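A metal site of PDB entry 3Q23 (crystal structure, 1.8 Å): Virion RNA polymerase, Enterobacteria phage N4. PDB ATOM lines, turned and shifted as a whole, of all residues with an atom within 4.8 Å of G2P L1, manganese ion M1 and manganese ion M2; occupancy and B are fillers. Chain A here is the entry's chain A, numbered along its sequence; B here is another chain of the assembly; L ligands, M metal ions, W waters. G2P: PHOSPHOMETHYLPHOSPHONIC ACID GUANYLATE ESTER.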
ATOM      1  N   ARG A 436     -19.297  -1.467  -5.592  1.00  0.00           N
ATOM      2  CA  ARG A 436     -20.646  -1.348  -6.141  1.00  0.00           C
ATOM      3  C   ARG A 436     -21.325  -0.073  -5.652  1.00  0.00           C
ATOM      4  O   ARG A 436     -21.120   0.342  -4.513  1.00  0.00           O
ATOM      5  CB  ARG A 436     -21.493  -2.571  -5.791  1.00  0.00           C
ATOM      6  CG  ARG A 436     -21.155  -3.791  -6.619  1.00  0.00           C
ATOM      7  CD  ARG A 436     -22.006  -4.958  -6.180  1.00  0.00           C
ATOM      8  NE  ARG A 436     -21.978  -6.043  -7.156  1.00  0.00           N
ATOM      9  CZ  ARG A 436     -22.664  -7.176  -7.003  1.00  0.00           C
ATOM     10  NH1 ARG A 436     -23.420  -7.354  -5.925  1.00  0.00           N
ATOM     11  NH2 ARG A 436     -22.593  -8.130  -7.928  1.00  0.00           N
ATOM     12  N   GLU A 569     -34.105  -4.525 -19.153  1.00  0.00           N
ATOM     13  CA  GLU A 569     -32.894  -4.718 -18.377  1.00  0.00           C
ATOM     14  C   GLU A 569     -31.826  -5.427 -19.196  1.00  0.00           C
ATOM     15  O   GLU A 569     -32.004  -6.599 -19.574  1.00  0.00           O
ATOM     16  CB  GLU A 569     -33.166  -5.528 -17.101  1.00  0.00           C
ATOM     17  CG  GLU A 569     -31.935  -5.684 -16.206  1.00  0.00           C
ATOM     18  CD  GLU A 569     -32.222  -6.394 -14.888  1.00  0.00           C
ATOM     19  OE1 GLU A 569     -31.348  -6.331 -14.004  1.00  0.00           O
ATOM     20  OE2 GLU A 569     -33.299  -7.009 -14.740  1.00  0.00           O
ATOM     21  N   ASP A 571     -28.681  -7.332 -18.811  1.00  0.00           N
ATOM     22  CA  ASP A 571     -28.071  -8.013 -17.670  1.00  0.00           C
ATOM     23  C   ASP A 571     -26.923  -8.913 -18.085  1.00  0.00           C
ATOM     24  O   ASP A 571     -26.983  -9.586 -19.125  1.00  0.00           O
ATOM     25  CB  ASP A 571     -29.113  -8.810 -16.863  1.00  0.00           C
ATOM     26  CG  ASP A 571     -28.538  -9.409 -15.591  1.00  0.00           C
ATOM     27  OD1 ASP A 571     -28.382  -8.662 -14.603  1.00  0.00           O
ATOM     28  OD2 ASP A 571     -28.234 -10.620 -15.567  1.00  0.00           O
ATOM     29  N   GLY A 572     -25.882  -8.923 -17.250  1.00  0.00           N
ATOM     30  CA  GLY A 572     -24.683  -9.715 -17.494  1.00  0.00           C
ATOM     31  C   GLY A 572     -24.959 -11.212 -17.483  1.00  0.00           C
ATOM     32  O   GLY A 572     -25.470 -11.753 -16.509  1.00  0.00           O
ATOM     33  N   VAL A 573     -24.621 -11.871 -18.592  1.00  0.00           N
ATOM     34  CA  VAL A 573     -24.820 -13.305 -18.725  1.00  0.00           C
ATOM     35  C   VAL A 573     -23.760 -14.038 -17.916  1.00  0.00           C
ATOM     36  O   VAL A 573     -22.570 -13.922 -18.204  1.00  0.00           O
ATOM     37  CB  VAL A 573     -24.779 -13.750 -20.205  1.00  0.00           C
ATOM     38  CG1 VAL A 573     -24.951 -15.263 -20.324  1.00  0.00           C
ATOM     39  CG2 VAL A 573     -25.839 -13.017 -21.014  1.00  0.00           C
ATOM     40  N   THR A 574     -24.199 -14.789 -16.905  1.00  0.00           N
ATOM     41  CA  THR A 574     -23.280 -15.505 -15.993  1.00  0.00           C
ATOM     42  C   THR A 574     -22.086 -14.608 -15.641  1.00  0.00           C
ATOM     43  O   THR A 574     -20.925 -14.968 -15.829  1.00  0.00           O
ATOM     44  CB  THR A 574     -22.867 -16.902 -16.562  1.00  0.00           C
ATOM     45  OG1 THR A 574     -22.045 -16.734 -17.717  1.00  0.00           O
ATOM     46  CG2 THR A 574     -24.100 -17.689 -16.969  1.00  0.00           C
ATOM     47  N   ASN A 575     -22.412 -13.432 -15.122  1.00  0.00           N
ATOM     48  CA  ASN A 575     -21.506 -12.277 -15.089  1.00  0.00           C
ATOM     49  C   ASN A 575     -20.190 -12.453 -14.314  1.00  0.00           C
ATOM     50  O   ASN A 575     -19.113 -12.301 -14.900  1.00  0.00           O
ATOM     51  CB  ASN A 575     -22.307 -11.043 -14.605  1.00  0.00           C
ATOM     52  CG  ASN A 575     -21.483  -9.775 -14.582  1.00  0.00           C
ATOM     53  OD1 ASN A 575     -21.334  -9.090 -15.609  1.00  0.00           O
ATOM     54  ND2 ASN A 575     -20.996  -9.424 -13.413  1.00  0.00           N
ATOM     55  N   GLY A 576     -20.295 -12.751 -13.022  1.00  0.00           N
ATOM     56  CA  GLY A 576     -19.120 -12.936 -12.171  1.00  0.00           C
ATOM     57  C   GLY A 576     -18.161 -13.986 -12.707  1.00  0.00           C
ATOM     58  O   GLY A 576     -16.967 -13.709 -12.890  1.00  0.00           O
ATOM     59  N   PRO A 577     -18.661 -15.217 -12.946  1.00  0.00           N
ATOM     60  CA  PRO A 577     -17.809 -16.259 -13.535  1.00  0.00           C
ATOM     61  C   PRO A 577     -17.111 -15.853 -14.841  1.00  0.00           C
ATOM     62  O   PRO A 577     -15.916 -16.089 -14.996  1.00  0.00           O
ATOM     63  CB  PRO A 577     -18.770 -17.424 -13.725  1.00  0.00           C
ATOM     64  CG  PRO A 577     -19.787 -17.224 -12.623  1.00  0.00           C
ATOM     65  CD  PRO A 577     -20.002 -15.734 -12.638  1.00  0.00           C
ATOM     66  N   TYR A 624     -23.465 -22.157 -16.895  1.00  0.00           N
ATOM     67  CA  TYR A 624     -24.031 -22.968 -15.821  1.00  0.00           C
ATOM     68  C   TYR A 624     -24.578 -24.300 -16.331  1.00  0.00           C
ATOM     69  O   TYR A 624     -24.369 -25.341 -15.693  1.00  0.00           O
ATOM     70  CB  TYR A 624     -25.074 -22.190 -15.016  1.00  0.00           C
ATOM     71  CG  TYR A 624     -24.568 -20.892 -14.403  1.00  0.00           C
ATOM     72  CD1 TYR A 624     -25.412 -19.778 -14.280  1.00  0.00           C
ATOM     73  CD2 TYR A 624     -23.249 -20.767 -13.972  1.00  0.00           C
ATOM     74  CE1 TYR A 624     -24.944 -18.582 -13.740  1.00  0.00           C
ATOM     75  CE2 TYR A 624     -22.778 -19.568 -13.424  1.00  0.00           C
ATOM     76  CZ  TYR A 624     -23.636 -18.490 -13.316  1.00  0.00           C
ATOM     77  OH  TYR A 624     -23.180 -17.302 -12.780  1.00  0.00           O
ATOM     78  N   ARG A 678     -29.626 -25.774 -15.648  1.00  0.00           N
ATOM     79  CA  ARG A 678     -28.583 -24.817 -15.238  1.00  0.00           C
ATOM     80  C   ARG A 678     -28.719 -24.342 -13.791  1.00  0.00           C
ATOM     81  O   ARG A 678     -27.725 -23.993 -13.154  1.00  0.00           O
ATOM     82  CB  ARG A 678     -28.578 -23.606 -16.176  1.00  0.00           C
ATOM     83  CG  ARG A 678     -29.777 -22.674 -15.982  1.00  0.00           C
ATOM     84  CD  ARG A 678     -29.832 -21.555 -17.010  1.00  0.00           C
ATOM     85  NE  ARG A 678     -28.840 -20.492 -16.788  1.00  0.00           N
ATOM     86  CZ  ARG A 678     -29.003 -19.466 -15.947  1.00  0.00           C
ATOM     87  NH1 ARG A 678     -30.092 -19.359 -15.199  1.00  0.00           N
ATOM     88  NH2 ARG A 678     -28.048 -18.553 -15.842  1.00  0.00           N
ATOM     89  N   LYS A 682     -25.850 -22.873 -10.908  1.00  0.00           N
ATOM     90  CA  LYS A 682     -25.765 -21.407 -10.927  1.00  0.00           C
ATOM     91  C   LYS A 682     -25.032 -20.822  -9.707  1.00  0.00           C
ATOM     92  O   LYS A 682     -23.965 -20.216  -9.858  1.00  0.00           O
ATOM     93  CB  LYS A 682     -27.158 -20.809 -11.081  1.00  0.00           C
ATOM     94  CG  LYS A 682     -27.240 -19.286 -10.952  1.00  0.00           C
ATOM     95  CD  LYS A 682     -28.520 -18.763 -11.585  1.00  0.00           C
ATOM     96  CE  LYS A 682     -28.936 -17.417 -11.033  1.00  0.00           C
ATOM     97  NZ  LYS A 682     -27.784 -16.522 -10.811  1.00  0.00           N
ATOM     98  N   ASN A 683     -25.584 -21.014  -8.517  1.00  0.00           N
ATOM     99  CA  ASN A 683     -24.946 -20.514  -7.313  1.00  0.00           C
ATOM    100  C   ASN A 683     -23.688 -21.283  -6.912  1.00  0.00           C
ATOM    101  O   ASN A 683     -22.678 -20.661  -6.591  1.00  0.00           O
ATOM    102  CB  ASN A 683     -25.932 -20.418  -6.143  1.00  0.00           C
ATOM    103  CG  ASN A 683     -25.390 -19.599  -4.990  1.00  0.00           C
ATOM    104  OD1 ASN A 683     -25.011 -20.137  -3.946  1.00  0.00           O
ATOM    105  ND2 ASN A 683     -25.316 -18.286  -5.174  1.00  0.00           N
ATOM    106  N   THR A 686     -20.734 -20.108  -9.027  1.00  0.00           N
ATOM    107  CA  THR A 686     -20.425 -18.726  -8.637  1.00  0.00           C
ATOM    108  C   THR A 686     -19.617 -18.675  -7.338  1.00  0.00           C
ATOM    109  O   THR A 686     -18.529 -18.097  -7.301  1.00  0.00           O
ATOM    110  CB  THR A 686     -21.728 -17.908  -8.479  1.00  0.00           C
ATOM    111  OG1 THR A 686     -22.436 -17.872  -9.718  1.00  0.00           O
ATOM    112  CG2 THR A 686     -21.423 -16.467  -8.037  1.00  0.00           C
ATOM    113  N   ILE A 687     -20.144 -19.319  -6.296  1.00  0.00           N
ATOM    114  CA  ILE A 687     -19.558 -19.186  -4.971  1.00  0.00           C
ATOM    115  C   ILE A 687     -18.309 -20.043  -4.781  1.00  0.00           C
ATOM    116  O   ILE A 687     -17.461 -19.735  -3.935  1.00  0.00           O
ATOM    117  CB  ILE A 687     -20.611 -19.351  -3.839  1.00  0.00           C
ATOM    118  CG1 ILE A 687     -21.056 -20.805  -3.661  1.00  0.00           C
ATOM    119  CG2 ILE A 687     -21.818 -18.435  -4.106  1.00  0.00           C
ATOM    120  CD1 ILE A 687     -21.824 -21.062  -2.372  1.00  0.00           C
ATOM    121  N   TYR A 690     -15.570 -17.951  -5.813  1.00  0.00           N
ATOM    122  CA  TYR A 690     -15.403 -16.974  -4.735  1.00  0.00           C
ATOM    123  C   TYR A 690     -14.897 -17.553  -3.399  1.00  0.00           C
ATOM    124  O   TYR A 690     -14.837 -16.841  -2.396  1.00  0.00           O
ATOM    125  CB  TYR A 690     -16.710 -16.199  -4.512  1.00  0.00           C
ATOM    126  CG  TYR A 690     -17.081 -15.276  -5.661  1.00  0.00           C
ATOM    127  CD1 TYR A 690     -18.399 -14.932  -5.893  1.00  0.00           C
ATOM    128  CD2 TYR A 690     -16.098 -14.759  -6.515  1.00  0.00           C
ATOM    129  CE1 TYR A 690     -18.752 -14.085  -6.942  1.00  0.00           C
ATOM    130  CE2 TYR A 690     -16.438 -13.916  -7.570  1.00  0.00           C
ATOM    131  CZ  TYR A 690     -17.760 -13.576  -7.775  1.00  0.00           C
ATOM    132  OH  TYR A 690     -18.103 -12.748  -8.811  1.00  0.00           O
ATOM    133  N   PRO A 933     -13.846 -12.558  -4.221  1.00  0.00           N
ATOM    134  CA  PRO A 933     -15.034 -11.760  -4.599  1.00  0.00           C
ATOM    135  C   PRO A 933     -14.806 -10.239  -4.570  1.00  0.00           C
ATOM    136  O   PRO A 933     -15.386  -9.533  -5.405  1.00  0.00           O
ATOM    137  CB  PRO A 933     -16.077 -12.178  -3.571  1.00  0.00           C
ATOM    138  CG  PRO A 933     -15.295 -12.718  -2.415  1.00  0.00           C
ATOM    139  CD  PRO A 933     -14.104 -13.379  -3.031  1.00  0.00           C
ATOM    140  N   ILE A 937     -15.843  -8.957  -8.192  1.00  0.00           N
ATOM    141  CA  ILE A 937     -16.993  -8.067  -8.243  1.00  0.00           C
ATOM    142  C   ILE A 937     -16.534  -6.649  -8.534  1.00  0.00           C
ATOM    143  O   ILE A 937     -17.090  -5.975  -9.405  1.00  0.00           O
ATOM    144  CB  ILE A 937     -17.842  -8.148  -6.940  1.00  0.00           C
ATOM    145  CG1 ILE A 937     -18.505  -9.526  -6.830  1.00  0.00           C
ATOM    146  CG2 ILE A 937     -18.889  -7.034  -6.924  1.00  0.00           C
ATOM    147  CD1 ILE A 937     -19.135  -9.832  -5.454  1.00  0.00           C
ATOM    148  N   ASP A 941     -18.162  -6.289 -12.468  1.00  0.00           N
ATOM    149  CA  ASP A 941     -19.419  -5.516 -12.542  1.00  0.00           C
ATOM    150  C   ASP A 941     -19.304  -4.098 -11.946  1.00  0.00           C
ATOM    151  O   ASP A 941     -19.898  -3.163 -12.478  1.00  0.00           O
ATOM    152  CB  ASP A 941     -20.643  -6.291 -12.002  1.00  0.00           C
ATOM    153  CG  ASP A 941     -20.649  -6.484 -10.480  1.00  0.00           C
ATOM    154  OD1 ASP A 941     -20.697  -5.482  -9.724  1.00  0.00           O
ATOM    155  OD2 ASP A 941     -20.663  -7.648 -10.037  1.00  0.00           O
ATOM    156  N   ILE A 961     -28.451  -2.032 -11.286  1.00  0.00           N
ATOM    157  CA  ILE A 961     -28.618  -3.068 -10.268  1.00  0.00           C
ATOM    158  C   ILE A 961     -27.446  -4.048 -10.372  1.00  0.00           C
ATOM    159  O   ILE A 961     -27.612  -5.254 -10.580  1.00  0.00           O
ATOM    160  CB  ILE A 961     -29.988  -3.792 -10.390  1.00  0.00           C
ATOM    161  CG1 ILE A 961     -31.124  -2.764 -10.534  1.00  0.00           C
ATOM    162  CG2 ILE A 961     -30.243  -4.687  -9.176  1.00  0.00           C
ATOM    163  CD1 ILE A 961     -32.393  -3.321 -11.157  1.00  0.00           C
ATOM    164  N   ASP A 963     -25.081  -5.886 -11.909  1.00  0.00           N
ATOM    165  CA  ASP A 963     -24.713  -6.403 -13.237  1.00  0.00           C
ATOM    166  C   ASP A 963     -25.840  -6.264 -14.261  1.00  0.00           C
ATOM    167  O   ASP A 963     -25.724  -6.752 -15.387  1.00  0.00           O
ATOM    168  CB  ASP A 963     -24.257  -7.853 -13.160  1.00  0.00           C
ATOM    169  CG  ASP A 963     -25.414  -8.819 -13.212  1.00  0.00           C
ATOM    170  OD1 ASP A 963     -26.372  -8.653 -12.411  1.00  0.00           O
ATOM    171  OD2 ASP A 963     -25.374  -9.737 -14.064  1.00  0.00           O
ATOM    172  N   GLY A 964     -26.927  -5.631 -13.842  1.00  0.00           N
ATOM    173  CA  GLY A 964     -28.058  -5.337 -14.719  1.00  0.00           C
ATOM    174  C   GLY A 964     -28.372  -3.860 -14.702  1.00  0.00           C
ATOM    175  O   GLY A 964     -28.167  -3.189 -13.689  1.00  0.00           O
ATOM    176  P    DC B  15     -17.869 -21.292   3.500  1.00  0.00           P
ATOM    177  OP1  DC B  15     -19.334 -21.235   3.705  1.00  0.00           O
ATOM    178  OP2  DC B  15     -16.973 -21.008   4.648  1.00  0.00           O
ATOM    179  O5'  DC B  15     -17.495 -20.235   2.368  1.00  0.00           O
ATOM    180  C5'  DC B  15     -17.709 -18.853   2.626  1.00  0.00           C
ATOM    181  C4'  DC B  15     -17.172 -18.048   1.452  1.00  0.00           C
ATOM    182  O4'  DC B  15     -17.797 -18.514   0.241  1.00  0.00           O
ATOM    183  C3'  DC B  15     -17.515 -16.569   1.530  1.00  0.00           C
ATOM    184  O3'  DC B  15     -16.543 -15.891   2.311  1.00  0.00           O
ATOM    185  C2'  DC B  15     -17.448 -16.181   0.049  1.00  0.00           C
ATOM    186  C1'  DC B  15     -18.140 -17.406  -0.576  1.00  0.00           C
ATOM    187  N1   DC B  15     -19.637 -17.287  -0.672  1.00  0.00           N
ATOM    188  C2   DC B  15     -20.178 -16.399  -1.615  1.00  0.00           C
ATOM    189  O2   DC B  15     -19.411 -15.748  -2.347  1.00  0.00           O
ATOM    190  N3   DC B  15     -21.530 -16.298  -1.697  1.00  0.00           N
ATOM    191  C4   DC B  15     -22.330 -17.013  -0.901  1.00  0.00           C
ATOM    192  N4   DC B  15     -23.656 -16.866  -1.036  1.00  0.00           N
ATOM    193  C5   DC B  15     -21.792 -17.918   0.061  1.00  0.00           C
ATOM    194  C6   DC B  15     -20.457 -18.019   0.140  1.00  0.00           C
ATOM    195  P    DC B  16     -17.002 -14.717   3.300  1.00  0.00           P
ATOM    196  OP1  DC B  16     -15.802 -14.316   4.060  1.00  0.00           O
ATOM    197  OP2  DC B  16     -18.235 -15.091   3.997  1.00  0.00           O
ATOM    198  O5'  DC B  16     -17.377 -13.538   2.286  1.00  0.00           O
ATOM    199  C5'  DC B  16     -16.327 -12.829   1.647  1.00  0.00           C
ATOM    200  C4'  DC B  16     -16.892 -11.771   0.727  1.00  0.00           C
ATOM    201  O4'  DC B  16     -17.684 -12.432  -0.282  1.00  0.00           O
ATOM    202  C3'  DC B  16     -17.874 -10.803   1.363  1.00  0.00           C
ATOM    203  O3'  DC B  16     -17.156  -9.787   2.061  1.00  0.00           O
ATOM    204  C2'  DC B  16     -18.577 -10.276   0.123  1.00  0.00           C
ATOM    205  C1'  DC B  16     -18.694 -11.549  -0.710  1.00  0.00           C
ATOM    206  N1   DC B  16     -20.048 -12.182  -0.590  1.00  0.00           N
ATOM    207  C2   DC B  16     -21.083 -11.718  -1.424  1.00  0.00           C
ATOM    208  O2   DC B  16     -20.857 -10.808  -2.227  1.00  0.00           O
ATOM    209  N3   DC B  16     -22.311 -12.281  -1.322  1.00  0.00           N
ATOM    210  C4   DC B  16     -22.537 -13.268  -0.444  1.00  0.00           C
ATOM    211  N4   DC B  16     -23.775 -13.774  -0.393  1.00  0.00           N
ATOM    212  C5   DC B  16     -21.507 -13.750   0.422  1.00  0.00           C
ATOM    213  C6   DC B  16     -20.296 -13.187   0.317  1.00  0.00           C
HETATM  214  PG  G2P L   1     -27.364 -14.909 -15.172  1.00  0.00           P
HETATM  215  O1G G2P L   1     -27.709 -13.436 -14.972  1.00  0.00           O
HETATM  216  O2G G2P L   1     -28.427 -15.814 -14.610  1.00  0.00           O
HETATM  217  O3G G2P L   1     -26.933 -15.252 -16.570  1.00  0.00           O
HETATM  218  O3B G2P L   1     -26.049 -15.228 -14.275  1.00  0.00           O
HETATM  219  PB  G2P L   1     -25.495 -14.263 -13.097  1.00  0.00           P
HETATM  220  O1B G2P L   1     -25.106 -12.949 -13.750  1.00  0.00           O
HETATM  221  O2B G2P L   1     -24.399 -15.017 -12.358  1.00  0.00           O
HETATM  222  C3A G2P L   1     -26.883 -14.069 -11.943  1.00  0.00           C
HETATM  223  PA  G2P L   1     -27.156 -12.380 -11.326  1.00  0.00           P
HETATM  224  O1A G2P L   1     -28.291 -12.428 -10.334  1.00  0.00           O
HETATM  225  O2A G2P L   1     -27.329 -11.457 -12.507  1.00  0.00           O
HETATM  226  O5' G2P L   1     -25.841 -11.984 -10.481  1.00  0.00           O
HETATM  227  C5' G2P L   1     -24.787 -11.224 -11.045  1.00  0.00           C
HETATM  228  C4' G2P L   1     -23.513 -11.396 -10.226  1.00  0.00           C
HETATM  229  O4' G2P L   1     -23.724 -11.050  -8.849  1.00  0.00           O
HETATM  230  C3' G2P L   1     -23.031 -12.837 -10.166  1.00  0.00           C
HETATM  231  O3' G2P L   1     -22.436 -13.325 -11.385  1.00  0.00           O
HETATM  232  C2' G2P L   1     -22.093 -12.761  -8.978  1.00  0.00           C
HETATM  233  O2' G2P L   1     -20.823 -12.208  -9.322  1.00  0.00           O
HETATM  234  C1' G2P L   1     -22.852 -11.836  -8.029  1.00  0.00           C
HETATM  235  N9  G2P L   1     -23.591 -12.759  -7.133  1.00  0.00           N
HETATM  236  C8  G2P L   1     -24.829 -13.270  -7.293  1.00  0.00           C
HETATM  237  N7  G2P L   1     -25.087 -14.124  -6.268  1.00  0.00           N
HETATM  238  C5  G2P L   1     -23.991 -14.154  -5.478  1.00  0.00           C
HETATM  239  C6  G2P L   1     -23.650 -14.825  -4.309  1.00  0.00           C
HETATM  240  O6  G2P L   1     -24.450 -15.607  -3.749  1.00  0.00           O
HETATM  241  N1  G2P L   1     -22.428 -14.613  -3.763  1.00  0.00           N
HETATM  242  C2  G2P L   1     -21.526 -13.780  -4.334  1.00  0.00           C
HETATM  243  N2  G2P L   1     -20.312 -13.587  -3.779  1.00  0.00           N
HETATM  244  N3  G2P L   1     -21.832 -13.121  -5.471  1.00  0.00           N
HETATM  245  C4  G2P L   1     -23.050 -13.290  -6.045  1.00  0.00           C
HETATM  246  PG  G2P L   2     -31.502  -9.673 -12.177  1.00  0.00           P
HETATM  247  O1G G2P L   2     -31.518  -8.164 -12.018  1.00  0.00           O
HETATM  248  O2G G2P L   2     -32.575 -10.198 -13.089  1.00  0.00           O
HETATM  249  O3G G2P L   2     -30.122 -10.242 -12.428  1.00  0.00           O
HETATM  250  O3B G2P L   2     -31.847 -10.133 -10.669  1.00  0.00           O
HETATM  251  PB  G2P L   2     -32.680 -11.438 -10.191  1.00  0.00           P
HETATM  252  O1B G2P L   2     -32.296 -12.595 -11.088  1.00  0.00           O
HETATM  253  O2B G2P L   2     -34.147 -11.053 -10.101  1.00  0.00           O
HETATM  254  C3A G2P L   2     -32.114 -11.795  -8.504  1.00  0.00           C
HETATM  255  PA  G2P L   2     -32.112 -10.355  -7.387  1.00  0.00           P
HETATM  256  O1A G2P L   2     -33.093  -9.322  -7.895  1.00  0.00           O
HETATM  257  O2A G2P L   2     -32.300 -10.918  -6.006  1.00  0.00           O
HETATM  258  O5' G2P L   2     -30.645  -9.705  -7.348  1.00  0.00           O
HETATM  259  C5' G2P L   2     -30.328  -8.446  -7.956  1.00  0.00           C
HETATM  260  C4' G2P L   2     -28.828  -8.350  -8.174  1.00  0.00           C
HETATM  261  O4' G2P L   2     -28.109  -8.177  -6.943  1.00  0.00           O
HETATM  262  C3' G2P L   2     -28.246  -9.619  -8.780  1.00  0.00           C
HETATM  263  O3' G2P L   2     -28.424  -9.718 -10.198  1.00  0.00           O
HETATM  264  C2' G2P L   2     -26.788  -9.539  -8.369  1.00  0.00           C
HETATM  265  O2' G2P L   2     -26.093  -8.637  -9.247  1.00  0.00           O
HETATM  266  C1' G2P L   2     -26.874  -8.924  -6.985  1.00  0.00           C
HETATM  267  N9  G2P L   2     -26.876  -9.987  -5.936  1.00  0.00           N
HETATM  268  C8  G2P L   2     -27.912 -10.765  -5.575  1.00  0.00           C
HETATM  269  N7  G2P L   2     -27.521 -11.605  -4.584  1.00  0.00           N
HETATM  270  C5  G2P L   2     -26.227 -11.355  -4.325  1.00  0.00           C
HETATM  271  C6  G2P L   2     -25.320 -11.892  -3.423  1.00  0.00           C
HETATM  272  O6  G2P L   2     -25.659 -12.811  -2.640  1.00  0.00           O
HETATM  273  N1  G2P L   2     -24.048 -11.402  -3.391  1.00  0.00           N
HETATM  274  C2  G2P L   2     -23.665 -10.410  -4.235  1.00  0.00           C
HETATM  275  N2  G2P L   2     -22.411  -9.932  -4.201  1.00  0.00           N
HETATM  276  N3  G2P L   2     -24.551  -9.882  -5.120  1.00  0.00           N
HETATM  277  C4  G2P L   2     -25.830 -10.328  -5.175  1.00  0.00           C
HETATM  278 MN    MN M   1     -26.489 -11.606 -14.632  1.00  0.00          MN
HETATM  279 MN    MN M   2     -28.270  -9.334 -12.572  1.00  0.00          MN
HETATM  280  O   HOH W   1     -29.110  -7.239 -11.782  1.00  0.00           O
HETATM  281  O   HOH W   2     -31.788 -16.037 -14.567  1.00  0.00           O
HETATM  282  O   HOH W   3     -26.803 -16.085  -2.662  1.00  0.00           O
HETATM  283  O   HOH W   4     -20.487 -10.100 -10.960  1.00  0.00           O
HETATM  284  O   HOH W   5     -30.207 -12.614 -14.093  1.00  0.00           O
HETATM  285  O   HOH W   6     -28.459 -15.015 -18.626  1.00  0.00           O
HETATM  286  O   HOH W   7     -28.687 -12.353 -18.071  1.00  0.00           O
HETATM  287  O   HOH W   8     -28.116 -13.406  -7.826  1.00  0.00           O
HETATM  288  O   HOH W   9     -30.209 -14.154 -10.775  1.00  0.00           O
HETATM  289  O   HOH W  10     -24.425 -16.036  -9.767  1.00  0.00           O
HETATM  290  O   HOH W  11     -27.739 -14.997  -5.666  1.00  0.00           O
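Of the 24 residues printed, 3 come within 4 Å of manganese ion M1. Along chain A the residues within 4 Å of manganese ion M1 span positions 571 to 963. The nearest printed residue that does not touch manganese ion M1 is Asn 575 (4.2 Å).
Water W1 lies within hydrogen-bond range of O1G of G2P L2 (2.6 Å), O of Ile 961 (2.8 Å), OE1 of Glu 569 (3.3 Å) and N of Gly 964 (3.4 Å). Water W9 lies within hydrogen-bond range of O1A of G2P L1 (2.6 Å), O1B of G2P L2 (2.6 Å) and NZ of Lys 682 (3.4 Å). Water W3 bridges an oxygen (O6) of G2P L1 (2.6 Å) and an oxygen (O6) of G2P L2 (3.5 Å). Water W4 lies within hydrogen-bond range of ND2 of Asn 575 (2.6 Å), OD2 of Asp 941 (2.6 Å), O2' of G2P L1 (2.7 Å) and N of Gly 576 (3.4 Å). Water W10 lies within hydrogen-bond range of the side-chain hydroxyl of Thr 686 (2.7 Å), an oxygen (O2B) of G2P L1 (2.8 Å) and the side-chain hydroxyl of Tyr 624 (3.5 Å).
Manganese ion M1 is bound by O1B of G2P L1 (2.1 Å), O of Gly 572 (2.1 Å), OD2 of Asp 571 (2.2 Å), O1G of G2P L1 (2.2 Å), OD2 of Asp 963 (2.2 Å) and O2A of G2P L1 (2.3 Å).
The side-chain hydroxyl (OH) of Tyr 624 is in hydrogen-bond range of an oxygen (O2B) of G2P L1. O2 of DC 15 of chain B is in hydrogen-bond range of N2 of G2P L1, at 2.7 Å. An oxygen (O3') of G2P L1 sits at hydrogen-bond distance from the backbone NH (N) of Gly 576, 2.8 Å away. The backbone NH of Thr 574 is in hydrogen-bond range of an oxygen (O3G) of G2P L1. The side-chain hydroxyl (OH) of Tyr 690 is in hydrogen-bond range of an oxygen (O2') of G2P L1 (2.8 Å). The side-chain amino group (NZ) of Lys 682 lies within salt-bridge range of an oxygen (O2G) of G2P L1, at 3.9 Å. O2G of G2P L1 is in salt-bridge range of NH2 of Arg 678 (3.0 Å). An oxygen (O1B) of G2P L1 lies close to the backbone NH of Asn 575, at 3.1 Å. A nitrogen (N2) of G2P L1 sits close to O2 of DC 16 of chain B (3.2 Å). O6 of G2P L1 sits at hydrogen-bond distance from ND2 of Asn 683. O4' of G2P L1 lies within hydrogen-bond range of NH2 of Arg 436, at 3.3 Å. N2 of G2P L2 is in hydrogen-bond range of O2 of DC 16 of chain B (2.7 Å). The guanidinium group (NH1) of Arg 436 sits at hydrogen-bond distance from a nitrogen (N3) of G2P L2 (2.9 Å). O1G of G2P L2 lies close to OE1 of Glu 569 (2.7 Å).
Val 573 touches G2P L1 (CA to O3G, 3.6 Å). Pro 577 touches G2P L1 (CD to O3', 3.6 Å). Thr 686 touches G2P L1. CG2 of Ile 687 touches O6 of G2P L1 (3.9 Å). Within 4 Å of G2P L1: Arg 436, Asp 571, Gly 572, Val 573, Thr 574, Asn 575, Gly 576, Pro 577, Tyr 624, Arg 678, Lys 682, Asn 683, Thr 686, Ile 687, Tyr 690, Asp 963, DC 15 of chain B and DC 16 of chain B.
Of the 24 residues printed, 2 come within 4 Å of manganese ion M2. Along chain A the residues within 4 Å of manganese ion M2 span positions 571 to 963. The nearest printed residue that does not touch manganese ion M2 is Gly 964 (4.1 Å).
OD1 of Asp 963 is bound to manganese ion M2, 2.0 Å away. An oxygen (O3G) of G2P L2 binds manganese ion M2, 2.1 Å away. OD1 of Asp 571 binds manganese ion M2 (2.1 Å). An oxygen (O2A) of G2P L1 is bound to manganese ion M2 (2.3 Å). Water W1 binds manganese ion M2 (2.4 Å). Manganese ion M2 is bound by O3' of G2P L2, at 2.4 Å. Manganese ion M2 has six donor atoms within binding distance.
OD1 of Asp 571 lies close to N of Gly 964 (3.4 Å). OG1 of Thr 686 is in hydrogen-bond range of OH of Tyr 624 (3.2 Å). O of Lys 682 is in hydrogen-bond range of OG1 of Thr 686 (2.8 Å). The guanidinium group of Arg 436 is in salt-bridge range of the side-chain carboxylate of Asp 941 (2.9 Å).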
